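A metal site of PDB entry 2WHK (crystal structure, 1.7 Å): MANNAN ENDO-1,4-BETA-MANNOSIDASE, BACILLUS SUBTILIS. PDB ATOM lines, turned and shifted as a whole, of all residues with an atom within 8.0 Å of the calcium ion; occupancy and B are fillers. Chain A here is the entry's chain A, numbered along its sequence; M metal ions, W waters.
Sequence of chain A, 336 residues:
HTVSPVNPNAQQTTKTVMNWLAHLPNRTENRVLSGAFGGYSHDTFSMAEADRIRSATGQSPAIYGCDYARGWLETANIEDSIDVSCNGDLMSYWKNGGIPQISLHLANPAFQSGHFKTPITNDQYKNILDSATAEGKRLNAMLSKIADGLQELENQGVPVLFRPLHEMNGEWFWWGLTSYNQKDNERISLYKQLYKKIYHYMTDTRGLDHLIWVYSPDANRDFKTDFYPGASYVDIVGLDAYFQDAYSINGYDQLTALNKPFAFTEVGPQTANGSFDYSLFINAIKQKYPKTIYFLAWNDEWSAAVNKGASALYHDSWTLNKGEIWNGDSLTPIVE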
ATOM      1  N   GLU A  29       9.062 -13.715  -7.143  1.00  0.00           N
ATOM      2  CA  GLU A  29       9.484 -13.535  -5.770  1.00  0.00           C
ATOM      3  C   GLU A  29       8.280 -13.181  -4.896  1.00  0.00           C
ATOM      4  O   GLU A  29       7.226 -12.798  -5.400  1.00  0.00           O
ATOM      5  CB  GLU A  29      10.554 -12.449  -5.670  1.00  0.00           C
ATOM      6  CG  GLU A  29      10.167 -11.114  -6.268  1.00  0.00           C
ATOM      7  CD  GLU A  29      11.169 -10.002  -5.962  1.00  0.00           C
ATOM      8  OE1 GLU A  29      12.343 -10.307  -5.659  1.00  0.00           O
ATOM      9  OE2 GLU A  29      10.773  -8.810  -6.033  1.00  0.00           O
ATOM     10  N   ASN A  30       8.462 -13.317  -3.587  1.00  0.00           N
ATOM     11  CA  ASN A  30       7.419 -13.015  -2.596  1.00  0.00           C
ATOM     12  C   ASN A  30       6.119 -13.701  -2.973  1.00  0.00           C
ATOM     13  O   ASN A  30       5.092 -13.074  -3.203  1.00  0.00           O
ATOM     14  CB  ASN A  30       7.231 -11.493  -2.458  1.00  0.00           C
ATOM     15  CG  ASN A  30       8.357 -10.844  -1.681  1.00  0.00           C
ATOM     16  OD1 ASN A  30       8.859 -11.411  -0.707  1.00  0.00           O
ATOM     17  ND2 ASN A  30       8.751  -9.632  -2.092  1.00  0.00           N
ATOM     18  N   ARG A  31       6.202 -15.032  -3.061  1.00  0.00           N
ATOM     19  CA  ARG A  31       5.093 -15.852  -3.530  1.00  0.00           C
ATOM     20  C   ARG A  31       4.684 -16.956  -2.556  1.00  0.00           C
ATOM     21  O   ARG A  31       3.730 -17.677  -2.836  1.00  0.00           O
ATOM     22  CB  ARG A  31       5.426 -16.464  -4.897  1.00  0.00           C
ATOM     23  CG  ARG A  31       6.765 -17.188  -4.969  1.00  0.00           C
ATOM     24  CD  ARG A  31       6.970 -17.735  -6.370  1.00  0.00           C
ATOM     25  NE  ARG A  31       6.144 -18.908  -6.610  1.00  0.00           N
ATOM     26  CZ  ARG A  31       6.010 -19.521  -7.787  1.00  0.00           C
ATOM     27  NH1 ARG A  31       6.607 -19.030  -8.885  1.00  0.00           N
ATOM     28  NH2 ARG A  31       5.239 -20.606  -7.881  1.00  0.00           N
ATOM     29  N   VAL A  32       5.374 -17.078  -1.413  1.00  0.00           N
ATOM     30  CA  VAL A  32       5.006 -18.016  -0.356  1.00  0.00           C
ATOM     31  C   VAL A  32       5.010 -17.278   0.984  1.00  0.00           C
ATOM     32  O   VAL A  32       6.063 -16.829   1.430  1.00  0.00           O
ATOM     33  CB  VAL A  32       5.993 -19.200  -0.257  1.00  0.00           C
ATOM     34  CG1 VAL A  32       5.577 -20.175   0.868  1.00  0.00           C
ATOM     35  CG2 VAL A  32       6.083 -19.937  -1.596  1.00  0.00           C
ATOM     36  N   SER A  34       5.277 -16.794   4.768  1.00  0.00           N
ATOM     37  CA  SER A  34       5.751 -17.473   5.958  1.00  0.00           C
ATOM     38  C   SER A  34       4.673 -17.472   7.033  1.00  0.00           C
ATOM     39  O   SER A  34       3.761 -16.628   7.037  1.00  0.00           O
ATOM     40  CB  SER A  34       7.013 -16.798   6.496  1.00  0.00           C
ATOM     41  OG  SER A  34       6.767 -15.411   6.688  1.00  0.00           O
ATOM     42  N   GLN A  59      13.098 -10.557  10.389  1.00  0.00           N
ATOM     43  CA  GLN A  59      11.790 -10.625   9.746  1.00  0.00           C
ATOM     44  C   GLN A  59      10.795 -11.336  10.661  1.00  0.00           C
ATOM     45  O   GLN A  59      11.189 -12.034  11.591  1.00  0.00           O
ATOM     46  CB  GLN A  59      11.893 -11.414   8.437  1.00  0.00           C
ATOM     47  CG  GLN A  59      12.902 -10.838   7.433  1.00  0.00           C
ATOM     48  CD  GLN A  59      12.519  -9.450   6.940  1.00  0.00           C
ATOM     49  OE1 GLN A  59      13.381  -8.560   6.803  1.00  0.00           O
ATOM     50  NE2 GLN A  59      11.238  -9.262   6.658  1.00  0.00           N
ATOM     51  N   LEU A 313      15.448 -19.633   5.106  1.00  0.00           N
ATOM     52  CA  LEU A 313      14.006 -19.745   4.867  1.00  0.00           C
ATOM     53  C   LEU A 313      13.377 -18.371   4.718  1.00  0.00           C
ATOM     54  O   LEU A 313      12.657 -18.110   3.759  1.00  0.00           O
ATOM     55  CB  LEU A 313      13.333 -20.496   6.023  1.00  0.00           C
ATOM     56  CG  LEU A 313      11.803 -20.644   5.990  1.00  0.00           C
ATOM     57  CD1 LEU A 313      11.361 -21.497   4.800  1.00  0.00           C
ATOM     58  CD2 LEU A 313      11.289 -21.237   7.297  1.00  0.00           C
ATOM     59  N   TYR A 314      13.661 -17.496   5.693  1.00  0.00           N
ATOM     60  CA  TYR A 314      13.024 -16.182   5.749  1.00  0.00           C
ATOM     61  C   TYR A 314      13.580 -15.201   4.725  1.00  0.00           C
ATOM     62  O   TYR A 314      12.869 -14.312   4.271  1.00  0.00           O
ATOM     63  CB  TYR A 314      13.077 -15.619   7.184  1.00  0.00           C
ATOM     64  CG  TYR A 314      11.855 -16.073   7.949  1.00  0.00           C
ATOM     65  CD1 TYR A 314      11.788 -17.353   8.489  1.00  0.00           C
ATOM     66  CD2 TYR A 314      10.740 -15.260   8.048  1.00  0.00           C
ATOM     67  CE1 TYR A 314      10.649 -17.785   9.149  1.00  0.00           C
ATOM     68  CE2 TYR A 314       9.602 -15.680   8.696  1.00  0.00           C
ATOM     69  CZ  TYR A 314       9.556 -16.943   9.247  1.00  0.00           C
ATOM     70  OH  TYR A 314       8.407 -17.344   9.888  1.00  0.00           O
ATOM     71  N   HIS A 315      14.843 -15.377   4.332  1.00  0.00           N
ATOM     72  CA  HIS A 315      15.455 -14.467   3.363  1.00  0.00           C
ATOM     73  C   HIS A 315      15.417 -14.982   1.929  1.00  0.00           C
ATOM     74  O   HIS A 315      15.774 -14.267   0.997  1.00  0.00           O
ATOM     75  CB  HIS A 315      16.876 -14.131   3.810  1.00  0.00           C
ATOM     76  CG  HIS A 315      16.919 -13.372   5.098  1.00  0.00           C
ATOM     77  ND1 HIS A 315      16.253 -12.177   5.260  1.00  0.00           N
ATOM     78  CD2 HIS A 315      17.526 -13.625   6.274  1.00  0.00           C
ATOM     79  CE1 HIS A 315      16.457 -11.727   6.489  1.00  0.00           C
ATOM     80  NE2 HIS A 315      17.214 -12.600   7.129  1.00  0.00           N
ATOM     81  N   ASP A 316      14.926 -16.211   1.746  1.00  0.00           N
ATOM     82  CA  ASP A 316      14.717 -16.733   0.391  1.00  0.00           C
ATOM     83  C   ASP A 316      13.865 -15.755  -0.430  1.00  0.00           C
ATOM     84  O   ASP A 316      12.892 -15.196   0.066  1.00  0.00           O
ATOM     85  CB  ASP A 316      14.044 -18.098   0.430  1.00  0.00           C
ATOM     86  CG  ASP A 316      14.148 -18.821  -0.894  1.00  0.00           C
ATOM     87  OD1 ASP A 316      13.382 -18.506  -1.824  1.00  0.00           O
ATOM     88  OD2 ASP A 316      15.024 -19.711  -0.990  1.00  0.00           O
ATOM     89  N   SER A 317      14.227 -15.566  -1.693  1.00  0.00           N
ATOM     90  CA  SER A 317      13.495 -14.626  -2.546  1.00  0.00           C
ATOM     91  C   SER A 317      12.000 -14.961  -2.696  1.00  0.00           C
ATOM     92  O   SER A 317      11.188 -14.081  -2.948  1.00  0.00           O
ATOM     93  CB  SER A 317      14.149 -14.530  -3.927  1.00  0.00           C
ATOM     94  OG  SER A 317      14.044 -15.771  -4.604  1.00  0.00           O
ATOM     95  N   TRP A 318      11.634 -16.230  -2.526  1.00  0.00           N
ATOM     96  CA  TRP A 318      10.233 -16.632  -2.639  1.00  0.00           C
ATOM     97  C   TRP A 318       9.399 -16.272  -1.405  1.00  0.00           C
ATOM     98  O   TRP A 318       8.169 -16.188  -1.475  1.00  0.00           O
ATOM     99  CB  TRP A 318      10.135 -18.140  -2.867  1.00  0.00           C
ATOM    100  CG  TRP A 318      10.414 -18.585  -4.272  1.00  0.00           C
ATOM    101  CD1 TRP A 318      11.403 -18.123  -5.097  1.00  0.00           C
ATOM    102  CD2 TRP A 318       9.713 -19.590  -4.996  1.00  0.00           C
ATOM    103  NE1 TRP A 318      11.344 -18.780  -6.305  1.00  0.00           N
ATOM    104  CE2 TRP A 318      10.312 -19.687  -6.266  1.00  0.00           C
ATOM    105  CE3 TRP A 318       8.626 -20.419  -4.704  1.00  0.00           C
ATOM    106  CZ2 TRP A 318       9.868 -20.577  -7.244  1.00  0.00           C
ATOM    107  CZ3 TRP A 318       8.178 -21.302  -5.659  1.00  0.00           C
ATOM    108  CH2 TRP A 318       8.796 -21.373  -6.917  1.00  0.00           C
ATOM    109  N   THR A 319      10.060 -16.073  -0.263  1.00  0.00           N
ATOM    110  CA  THR A 319       9.356 -15.950   1.009  1.00  0.00           C
ATOM    111  C   THR A 319       8.817 -14.534   1.235  1.00  0.00           C
ATOM    112  O   THR A 319       9.572 -13.558   1.199  1.00  0.00           O
ATOM    113  CB  THR A 319      10.243 -16.399   2.176  1.00  0.00           C
ATOM    114  OG1 THR A 319      10.775 -17.690   1.871  1.00  0.00           O
ATOM    115  CG2 THR A 319       9.447 -16.474   3.478  1.00  0.00           C
ATOM    116  N   LEU A 320       7.509 -14.462   1.466  1.00  0.00           N
ATOM    117  CA  LEU A 320       6.803 -13.205   1.698  1.00  0.00           C
ATOM    118  C   LEU A 320       6.506 -13.120   3.194  1.00  0.00           C
ATOM    119  O   LEU A 320       5.832 -13.972   3.761  1.00  0.00           O
ATOM    120  CB  LEU A 320       5.513 -13.180   0.878  1.00  0.00           C
ATOM    121  CG  LEU A 320       4.741 -11.864   0.775  1.00  0.00           C
ATOM    122  CD1 LEU A 320       3.763 -11.920  -0.383  1.00  0.00           C
ATOM    123  CD2 LEU A 320       4.009 -11.510   2.094  1.00  0.00           C
ATOM    124  N   ASN A 321       7.034 -12.083   3.831  1.00  0.00           N
ATOM    125  CA  ASN A 321       7.022 -11.964   5.283  1.00  0.00           C
ATOM    126  C   ASN A 321       6.131 -10.834   5.737  1.00  0.00           C
ATOM    127  O   ASN A 321       5.598 -10.092   4.902  1.00  0.00           O
ATOM    128  CB  ASN A 321       8.449 -11.772   5.789  1.00  0.00           C
ATOM    129  CG  ASN A 321       9.310 -12.992   5.539  1.00  0.00           C
ATOM    130  OD1 ASN A 321       8.897 -14.112   5.844  1.00  0.00           O
ATOM    131  ND2 ASN A 321      10.493 -12.799   4.958  1.00  0.00           N
ATOM    132  N   LYS A 322       5.948 -10.706   7.037  1.00  0.00           N
ATOM    133  CA  LYS A 322       5.178  -9.598   7.602  1.00  0.00           C
ATOM    134  C   LYS A 322       5.706  -8.284   7.015  1.00  0.00           C
ATOM    135  O   LYS A 322       6.916  -8.080   6.949  1.00  0.00           O
ATOM    136  CB  LYS A 322       5.294  -9.591   9.122  1.00  0.00           C
ATOM    137  CG  LYS A 322       4.211  -8.812   9.856  1.00  0.00           C
ATOM    138  CD  LYS A 322       4.520  -8.784  11.353  1.00  0.00           C
ATOM    139  CE  LYS A 322       3.418  -8.153  12.191  1.00  0.00           C
ATOM    140  NZ  LYS A 322       3.849  -8.019  13.616  1.00  0.00           N
ATOM    141  N   GLU A 324       5.234  -7.396   3.846  1.00  0.00           N
ATOM    142  CA  GLU A 324       5.309  -7.556   2.389  1.00  0.00           C
ATOM    143  C   GLU A 324       3.956  -7.842   1.732  1.00  0.00           C
ATOM    144  O   GLU A 324       3.889  -8.147   0.523  1.00  0.00           O
ATOM    145  CB  GLU A 324       6.333  -8.648   2.026  1.00  0.00           C
ATOM    146  CG  GLU A 324       7.753  -8.331   2.453  1.00  0.00           C
ATOM    147  CD  GLU A 324       8.768  -9.332   1.925  1.00  0.00           C
ATOM    148  OE1 GLU A 324       8.741 -10.507   2.342  1.00  0.00           O
ATOM    149  OE2 GLU A 324       9.620  -8.951   1.090  1.00  0.00           O
HETATM  150 CA    CA M   1      10.570 -11.420   0.988  1.00  0.00          CA
HETATM  151  O   HOH W   1      11.693 -11.992  -1.072  1.00  0.00           O
HETATM  152  O   HOH W   2      12.533 -12.927   1.656  1.00  0.00           O
HETATM  153  O   HOH W   3      12.562  -9.847   0.645  1.00  0.00           O
HETATM  154  O   HOH W   4      11.421 -10.607   3.203  1.00  0.00           O
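O of Thr 319 binds the calcium ion (2.4 Å). The calcium ion is bound by OD1 of Asn 30, 2.4 Å away. The calcium ion is bound by water W1 (2.4 Å). OE1 of Glu 324 binds the calcium ion, 2.5 Å away. Water W4 is bound to the calcium ion (2.5 Å). Water W3 binds the calcium ion, at 2.6 Å. The calcium ion is bound by water W2 (2.6 Å). OE2 of Glu 324 is bound to the calcium ion (2.6 Å). The calcium ion has eight donor atoms within binding distance.
The side-chain hydroxyl of Thr 319 sits at hydrogen-bond distance from the backbone carbonyl oxygen of Leu 313, 2.7 Å away. O of Ser 317 sits at hydrogen-bond distance from N of Asn 30 (2.9 Å). The side-chain carboxylate of Glu 324 lies close to the backbone NH of Asn 321 (2.8 Å).
Within 4 Å of the calcium ion: Asn 30, Thr 319 and Glu 324. The nearest printed residue that does not touch the calcium ion is Asn 321 (4.2 Å).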
